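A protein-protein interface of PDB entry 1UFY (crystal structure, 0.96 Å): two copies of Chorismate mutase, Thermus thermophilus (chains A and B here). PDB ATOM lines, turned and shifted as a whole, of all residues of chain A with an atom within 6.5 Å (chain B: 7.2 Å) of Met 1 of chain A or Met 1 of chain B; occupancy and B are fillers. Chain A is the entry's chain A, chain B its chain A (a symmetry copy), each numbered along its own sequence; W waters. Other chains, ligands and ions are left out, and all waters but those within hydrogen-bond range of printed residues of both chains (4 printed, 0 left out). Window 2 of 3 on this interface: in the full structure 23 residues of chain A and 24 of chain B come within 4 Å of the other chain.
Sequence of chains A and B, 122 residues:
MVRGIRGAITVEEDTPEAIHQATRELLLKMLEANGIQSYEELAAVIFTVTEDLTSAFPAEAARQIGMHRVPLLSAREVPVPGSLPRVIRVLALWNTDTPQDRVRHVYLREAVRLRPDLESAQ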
ATOM      1  N   MET A   1      -6.643  -1.517  18.347  1.00  0.00           N
ATOM      2  CA  MET A   1      -6.129  -0.207  18.690  1.00  0.00           C
ATOM      3  C   MET A   1      -6.593   0.831  17.617  1.00  0.00           C
ATOM      4  O   MET A   1      -6.867   0.591  16.431  1.00  0.00           O
ATOM      5  CB  MET A   1      -4.662  -0.031  18.806  1.00  0.00           C
ATOM      6  CG  MET A   1      -3.899  -0.095  17.505  1.00  0.00           C
ATOM      7  SD  MET A   1      -2.210   0.530  17.939  1.00  0.00           S
ATOM      8  CE  MET A   1      -2.728   2.263  17.824  1.00  0.00           C
ATOM      9  N   VAL A   2      -6.770   1.966  18.231  1.00  0.00           N
ATOM     10  CA  VAL A   2      -7.493   3.071  17.600  1.00  0.00           C
ATOM     11  C   VAL A   2      -6.639   4.334  17.701  1.00  0.00           C
ATOM     12  O   VAL A   2      -5.992   4.583  18.707  1.00  0.00           O
ATOM     13  CB  VAL A   2      -8.856   3.280  18.288  1.00  0.00           C
ATOM     14  CG1 VAL A   2      -9.557   4.516  17.799  1.00  0.00           C
ATOM     15  CG2 VAL A   2      -9.646   1.971  18.096  1.00  0.00           C
ATOM     16  N   ARG A   3      -6.705   5.137  16.652  1.00  0.00           N
ATOM     17  CA  ARG A   3      -6.132   6.474  16.644  1.00  0.00           C
ATOM     18  C   ARG A   3      -7.222   7.472  16.309  1.00  0.00           C
ATOM     19  O   ARG A   3      -7.910   7.346  15.295  1.00  0.00           O
ATOM     20  CB  ARG A   3      -5.023   6.611  15.589  1.00  0.00           C
ATOM     21  CG  ARG A   3      -3.772   5.795  15.891  1.00  0.00           C
ATOM     22  CD  ARG A   3      -3.078   6.338  17.082  1.00  0.00           C
ATOM     23  NE  ARG A   3      -1.844   5.581  17.401  1.00  0.00           N
ATOM     24  CZ  ARG A   3      -1.317   5.567  18.614  1.00  0.00           C
ATOM     25  NH1 ARG A   3      -1.831   6.291  19.586  1.00  0.00           N
ATOM     26  NH2 ARG A   3      -0.254   4.826  18.835  1.00  0.00           N
ATOM     27  N   GLU A  40     -14.561   1.410   6.036  1.00  0.00           N
ATOM     28  CA  GLU A  40     -14.554   0.331   6.997  1.00  0.00           C
ATOM     29  C   GLU A  40     -13.472   0.481   8.044  1.00  0.00           C
ATOM     30  O   GLU A  40     -13.528  -0.145   9.096  1.00  0.00           O
ATOM     31  CB  GLU A  40     -14.348  -1.008   6.262  1.00  0.00           C
ATOM     32  CG  GLU A  40     -15.525  -1.356   5.346  1.00  0.00           C
ATOM     33  CD  GLU A  40     -15.175  -2.400   4.346  1.00  0.00           C
ATOM     34  OE1 GLU A  40     -14.160  -2.217   3.535  1.00  0.00           O
ATOM     35  OE2 GLU A  40     -15.934  -3.363   4.269  1.00  0.00           O
ATOM     36  N   ALA A  43     -14.017   3.415  12.980  1.00  0.00           N
ATOM     37  CA  ALA A  43     -14.851   2.934  14.080  1.00  0.00           C
ATOM     38  C   ALA A  43     -16.106   3.785  14.225  1.00  0.00           C
ATOM     39  O   ALA A  43     -17.217   3.270  14.452  1.00  0.00           O
ATOM     40  CB  ALA A  43     -14.072   2.920  15.363  1.00  0.00           C
ATOM     41  N   TRP A  94     -10.161   5.914  14.190  1.00  0.00           N
ATOM     42  CA  TRP A  94      -9.584   5.122  13.082  1.00  0.00           C
ATOM     43  C   TRP A  94      -8.953   3.852  13.614  1.00  0.00           C
ATOM     44  O   TRP A  94      -8.080   3.887  14.476  1.00  0.00           O
ATOM     45  CB  TRP A  94      -8.562   6.008  12.400  1.00  0.00           C
ATOM     46  CG  TRP A  94      -7.836   5.428  11.238  1.00  0.00           C
ATOM     47  CD1 TRP A  94      -8.211   4.435  10.407  1.00  0.00           C
ATOM     48  CD2 TRP A  94      -6.545   5.876  10.756  1.00  0.00           C
ATOM     49  NE1 TRP A  94      -7.244   4.218   9.448  1.00  0.00           N
ATOM     50  CE2 TRP A  94      -6.222   5.103   9.654  1.00  0.00           C
ATOM     51  CE3 TRP A  94      -5.658   6.867  11.196  1.00  0.00           C
ATOM     52  CZ2 TRP A  94      -5.048   5.289   8.967  1.00  0.00           C
ATOM     53  CZ3 TRP A  94      -4.487   7.049  10.497  1.00  0.00           C
ATOM     54  CH2 TRP A  94      -4.194   6.271   9.402  1.00  0.00           C
ATOM     55  N   ASN A  95      -9.417   2.680  13.129  1.00  0.00           N
ATOM     56  CA  ASN A  95      -8.814   1.407  13.465  1.00  0.00           C
ATOM     57  C   ASN A  95      -7.527   1.234  12.654  1.00  0.00           C
ATOM     58  O   ASN A  95      -7.581   1.018  11.446  1.00  0.00           O
ATOM     59  CB  ASN A  95      -9.775   0.274  13.131  1.00  0.00           C
ATOM     60  CG  ASN A  95     -10.965   0.215  14.041  1.00  0.00           C
ATOM     61  OD1 ASN A  95     -10.814   0.246  15.255  1.00  0.00           O
ATOM     62  ND2 ASN A  95     -12.149   0.124  13.504  1.00  0.00           N
ATOM     63  N   THR A  96      -6.386   1.405  13.310  1.00  0.00           N
ATOM     64  CA  THR A  96      -5.105   1.434  12.656  1.00  0.00           C
ATOM     65  C   THR A  96      -4.019   1.170  13.727  1.00  0.00           C
ATOM     66  O   THR A  96      -4.230   1.509  14.898  1.00  0.00           O
ATOM     67  CB  THR A  96      -4.861   2.768  11.964  1.00  0.00           C
ATOM     68  OG1 THR A  96      -3.644   2.695  11.199  1.00  0.00           O
ATOM     69  CG2 THR A  96      -4.723   3.920  12.959  1.00  0.00           C
ATOM     70  N   ASP A  97      -2.867   0.697  13.233  1.00  0.00           N
ATOM     71  CA  ASP A  97      -1.695   0.642  14.113  1.00  0.00           C
ATOM     72  C   ASP A  97      -0.727   1.779  13.801  1.00  0.00           C
ATOM     73  O   ASP A  97       0.375   1.806  14.314  1.00  0.00           O
ATOM     74  CB  ASP A  97      -1.022  -0.697  14.083  1.00  0.00           C
ATOM     75  CG  ASP A  97      -0.544  -1.073  12.733  1.00  0.00           C
ATOM     76  OD1 ASP A  97      -0.607  -0.290  11.820  1.00  0.00           O
ATOM     77  OD2 ASP A  97      -0.066  -2.231  12.613  1.00  0.00           O
ATOM     78  N   THR A  98      -1.130   2.764  13.005  1.00  0.00           N
ATOM     79  CA  THR A  98      -0.307   3.936  12.727  1.00  0.00           C
ATOM     80  C   THR A  98       0.160   4.572  14.021  1.00  0.00           C
ATOM     81  O   THR A  98      -0.644   4.844  14.900  1.00  0.00           O
ATOM     82  CB  THR A  98      -1.131   4.970  11.931  1.00  0.00           C
ATOM     83  OG1 THR A  98      -1.589   4.365  10.699  1.00  0.00           O
ATOM     84  CG2 THR A  98      -0.344   6.183  11.595  1.00  0.00           C
ATOM     85  N   PRO A  99       1.463   4.878  14.144  1.00  0.00           N
ATOM     86  CA  PRO A  99       1.930   5.585  15.313  1.00  0.00           C
ATOM     87  C   PRO A  99       1.283   6.939  15.489  1.00  0.00           C
ATOM     88  O   PRO A  99       0.928   7.597  14.524  1.00  0.00           O
ATOM     89  CB  PRO A  99       3.440   5.739  15.043  1.00  0.00           C
ATOM     90  CG  PRO A  99       3.773   4.647  14.104  1.00  0.00           C
ATOM     91  CD  PRO A  99       2.559   4.462  13.272  1.00  0.00           C
ATOM     92  N   MET B   1      -9.450  -3.268  17.771  1.00  0.00           N
ATOM     93  CA  MET B   1     -10.357  -2.637  16.834  1.00  0.00           C
ATOM     94  C   MET B   1     -11.795  -2.600  17.445  1.00  0.00           C
ATOM     95  O   MET B   1     -12.260  -3.389  18.281  1.00  0.00           O
ATOM     96  CB  MET B   1     -10.512  -3.236  15.488  1.00  0.00           C
ATOM     97  CG  MET B   1     -11.240  -4.558  15.449  1.00  0.00           C
ATOM     98  SD  MET B   1     -11.593  -4.829  13.650  1.00  0.00           S
ATOM     99  CE  MET B   1     -13.053  -3.755  13.687  1.00  0.00           C
ATOM    100  N   VAL B   2     -12.367  -1.511  17.018  1.00  0.00           N
ATOM    101  CA  VAL B   2     -13.595  -1.002  17.629  1.00  0.00           C
ATOM    102  C   VAL B   2     -14.618  -0.738  16.524  1.00  0.00           C
ATOM    103  O   VAL B   2     -14.283  -0.263  15.450  1.00  0.00           O
ATOM    104  CB  VAL B   2     -13.303   0.289  18.419  1.00  0.00           C
ATOM    105  CG1 VAL B   2     -14.559   0.950  18.914  1.00  0.00           C
ATOM    106  CG2 VAL B   2     -12.298  -0.094  19.523  1.00  0.00           C
ATOM    107  N   ARG B   3     -15.871  -1.013  16.849  1.00  0.00           N
ATOM    108  CA  ARG B   3     -17.002  -0.639  16.013  1.00  0.00           C
ATOM    109  C   ARG B   3     -17.954   0.210  16.832  1.00  0.00           C
ATOM    110  O   ARG B   3     -18.393  -0.187  17.913  1.00  0.00           O
ATOM    111  CB  ARG B   3     -17.773  -1.871  15.516  1.00  0.00           C
ATOM    112  CG  ARG B   3     -16.997  -2.734  14.530  1.00  0.00           C
ATOM    113  CD  ARG B   3     -16.800  -2.007  13.254  1.00  0.00           C
ATOM    114  NE  ARG B   3     -16.061  -2.821  12.257  1.00  0.00           N
ATOM    115  CZ  ARG B   3     -15.386  -2.275  11.259  1.00  0.00           C
ATOM    116  NH1 ARG B   3     -15.400  -0.974  11.063  1.00  0.00           N
ATOM    117  NH2 ARG B   3     -14.709  -3.057  10.450  1.00  0.00           N
ATOM    118  N   TRP B  94     -17.731  -0.491  20.706  1.00  0.00           N
ATOM    119  CA  TRP B  94     -17.743  -1.953  20.928  1.00  0.00           C
ATOM    120  C   TRP B  94     -16.431  -2.565  20.483  1.00  0.00           C
ATOM    121  O   TRP B  94     -16.013  -2.415  19.338  1.00  0.00           O
ATOM    122  CB  TRP B  94     -18.911  -2.505  20.138  1.00  0.00           C
ATOM    123  CG  TRP B  94     -19.135  -3.974  20.202  1.00  0.00           C
ATOM    124  CD1 TRP B  94     -18.775  -4.850  21.162  1.00  0.00           C
ATOM    125  CD2 TRP B  94     -19.844  -4.752  19.208  1.00  0.00           C
ATOM    126  NE1 TRP B  94     -19.193  -6.123  20.833  1.00  0.00           N
ATOM    127  CE2 TRP B  94     -19.855  -6.067  19.638  1.00  0.00           C
ATOM    128  CE3 TRP B  94     -20.453  -4.412  17.992  1.00  0.00           C
ATOM    129  CZ2 TRP B  94     -20.461  -7.057  18.904  1.00  0.00           C
ATOM    130  CZ3 TRP B  94     -21.062  -5.410  17.267  1.00  0.00           C
ATOM    131  CH2 TRP B  94     -21.062  -6.708  17.722  1.00  0.00           C
ATOM    132  N   ASN B  95     -15.722  -3.249  21.407  1.00  0.00           N
ATOM    133  CA  ASN B  95     -14.517  -3.983  21.075  1.00  0.00           C
ATOM    134  C   ASN B  95     -14.905  -5.300  20.397  1.00  0.00           C
ATOM    135  O   ASN B  95     -15.413  -6.206  21.050  1.00  0.00           O
ATOM    136  CB  ASN B  95     -13.728  -4.284  22.343  1.00  0.00           C
ATOM    137  CG  ASN B  95     -13.099  -3.068  22.955  1.00  0.00           C
ATOM    138  OD1 ASN B  95     -12.440  -2.302  22.265  1.00  0.00           O
ATOM    139  ND2 ASN B  95     -13.268  -2.861  24.230  1.00  0.00           N
ATOM    140  N   THR B  96     -14.731  -5.362  19.082  1.00  0.00           N
ATOM    141  CA  THR B  96     -15.194  -6.465  18.283  1.00  0.00           C
ATOM    142  C   THR B  96     -14.424  -6.436  16.940  1.00  0.00           C
ATOM    143  O   THR B  96     -14.024  -5.352  16.497  1.00  0.00           O
ATOM    144  CB  THR B  96     -16.695  -6.388  18.042  1.00  0.00           C
ATOM    145  OG1 THR B  96     -17.134  -7.585  17.375  1.00  0.00           O
ATOM    146  CG2 THR B  96     -17.080  -5.193  17.168  1.00  0.00           C
ATOM    147  N   ASP B  97     -14.377  -7.616  16.311  1.00  0.00           N
ATOM    148  CA  ASP B  97     -13.892  -7.657  14.927  1.00  0.00           C
ATOM    149  C   ASP B  97     -15.053  -7.799  13.948  1.00  0.00           C
ATOM    150  O   ASP B  97     -14.840  -8.011  12.770  1.00  0.00           O
ATOM    151  CB  ASP B  97     -12.846  -8.710  14.721  1.00  0.00           C
ATOM    152  CG  ASP B  97     -13.332 -10.075  15.029  1.00  0.00           C
ATOM    153  OD1 ASP B  97     -14.491 -10.268  15.293  1.00  0.00           O
ATOM    154  OD2 ASP B  97     -12.475 -10.995  14.981  1.00  0.00           O
ATOM    155  N   THR B  98     -16.293  -7.631  14.396  1.00  0.00           N
ATOM    156  CA  THR B  98     -17.456  -7.657  13.514  1.00  0.00           C
ATOM    157  C   THR B  98     -17.265  -6.694  12.360  1.00  0.00           C
ATOM    158  O   THR B  98     -16.944  -5.534  12.571  1.00  0.00           O
ATOM    159  CB  THR B  98     -18.714  -7.244  14.306  1.00  0.00           C
ATOM    160  OG1 THR B  98     -18.895  -8.154  15.417  1.00  0.00           O
ATOM    161  CG2 THR B  98     -19.942  -7.269  13.471  1.00  0.00           C
ATOM    162  N   PRO B  99     -17.513  -7.136  11.116  1.00  0.00           N
ATOM    163  CA  PRO B  99     -17.452  -6.223   9.999  1.00  0.00           C
ATOM    164  C   PRO B  99     -18.427  -5.075  10.114  1.00  0.00           C
ATOM    165  O   PRO B  99     -19.499  -5.215  10.683  1.00  0.00           O
ATOM    166  CB  PRO B  99     -17.810  -7.119   8.799  1.00  0.00           C
ATOM    167  CG  PRO B  99     -17.467  -8.491   9.230  1.00  0.00           C
ATOM    168  CD  PRO B  99     -17.726  -8.519  10.690  1.00  0.00           C
ATOM    169  N   GLN B 100     -18.075  -3.937   9.529  1.00  0.00           N
ATOM    170  CA  GLN B 100     -18.891  -2.765   9.592  1.00  0.00           C
ATOM    171  C   GLN B 100     -20.312  -3.001   9.110  1.00  0.00           C
ATOM    172  O   GLN B 100     -21.279  -2.456   9.714  1.00  0.00           O
ATOM    173  CB  GLN B 100     -18.237  -1.640   8.785  1.00  0.00           C
ATOM    174  CG  GLN B 100     -18.897  -0.295   8.938  1.00  0.00           C
ATOM    175  CD  GLN B 100     -18.080   0.807   8.273  1.00  0.00           C
ATOM    176  OE1 GLN B 100     -18.051   0.897   7.056  1.00  0.00           O
ATOM    177  NE2 GLN B 100     -17.349   1.589   9.059  1.00  0.00           N
HETATM  178  O   HOH W   1     -15.834  -4.192   7.543  1.00  0.00           O
HETATM  179  O   HOH W   2     -11.730  -1.307  10.884  1.00  0.00           O
HETATM  180  O   HOH W   3     -17.387   0.976  11.999  1.00  0.00           O
HETATM  181  O   HOH W   4     -18.408  -4.533   6.241  1.00  0.00           O
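Met 1 of chain A touches just one residue of chain B: Met 1 (3.4 Å). Met 1 of chain B touches two residues of chain A. Printed residues of chain B within 4 Å of Glu 40 of chain A: Arg 3 (2.8 Å) and Gln 100 (3.5 Å). Printed residues of chain B within 4 Å of Ala 43 of chain A: Val 2 and Arg 3. Pro 99 of chain B touches none of the printed residues of chain A. The nearest printed residue of chain B that does not touch Asn 95 of chain A is Arg 3 of chain B (4.2 Å).
Of the 11 printed residues of chain A, 5 touch a printed residue of chain B. Hydrophobic or aromatic side chains of chain A within 4 Å of the printed part of chain B: Val 2 and Ala 43.
O of Glu 40 of chain A sits at hydrogen-bond distance from NH1 of Arg 3 of chain B (2.8 Å). The backbone NH (N) of Met 1 of chain A sits close to the backbone NH (N) of Met 1 of chain B (3.4 Å). ND2 of Asn 95 of chain A sits at hydrogen-bond distance from O of Val 2 of chain B.
The backbone carbonyl oxygen (O) of Met 1 of chain B sits at hydrogen-bond distance from the backbone NH (N) of Thr 96 of chain B (3.3 Å). O of Met 1 of chain A sits at hydrogen-bond distance from N of Thr 96 of chain A. O of Thr 98 of chain B is in hydrogen-bond range of NE of Arg 3 of chain B. O of Trp 94 of chain B lies within hydrogen-bond range of N of Arg 3 of chain B.
Water W2 lies within hydrogen-bond range of O of Glu 40 of chain A (2.8 Å), ND2 of Asn 95 of chain A (3.0 Å) and NH2 of Arg 3 of chain B (3.5 Å). Water W3 lies within hydrogen-bond range of NH1 of Arg 3 of chain B (2.9 Å), NE2 of Gln 100 of chain B (3.0 Å) and O of Ala 43 of chain A (3.4 Å). Water W1 lies within hydrogen-bond range of the backbone NH of Gln 100 of chain B (3.0 Å), the guanidinium group of Arg 3 of chain B (3.3 Å) and the side-chain carboxylate of Glu 40 of chain A (3.4 Å). Water W4 lies within hydrogen-bond range of the backbone NH of Gln 100 of chain B (3.4 Å) and the side-chain carboxylate of Glu 40 of chain A (3.4 Å).
Met 1 of chain A touches its own counterpart, Met 1 of chain B. Val 2 of chain A touches its own counterpart, Val 2 of chain B. Asn 95 of chain A touches Met 1 of chain B, but with the chains exchanged Met 1 of chain A does not touch Asn 95 of chain B (7.0 Å). Asn 95 of chain A touches Val 2 of chain B, but with the chains exchanged Val 2 of chain A does not touch Asn 95 of chain B (6.6 Å). Positions printed for both chains: 1, 2, 3, 94, 95, 96, 97, 98 and 99.
Among the printed residues, pairs that only touch across the chains: Val 2 of chain A with Val 2 of chain B (3.7 Å), Glu 40 of chain A with Gln 100 of chain B (3.5 Å), Ala 43 of chain A with Val 2 of chain B (3.2 Å), Ala 43 of chain A with Arg 3 of chain B (3.9 Å) and Asn 95 of chain A with Met 1 of chain B (3.3 Å).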
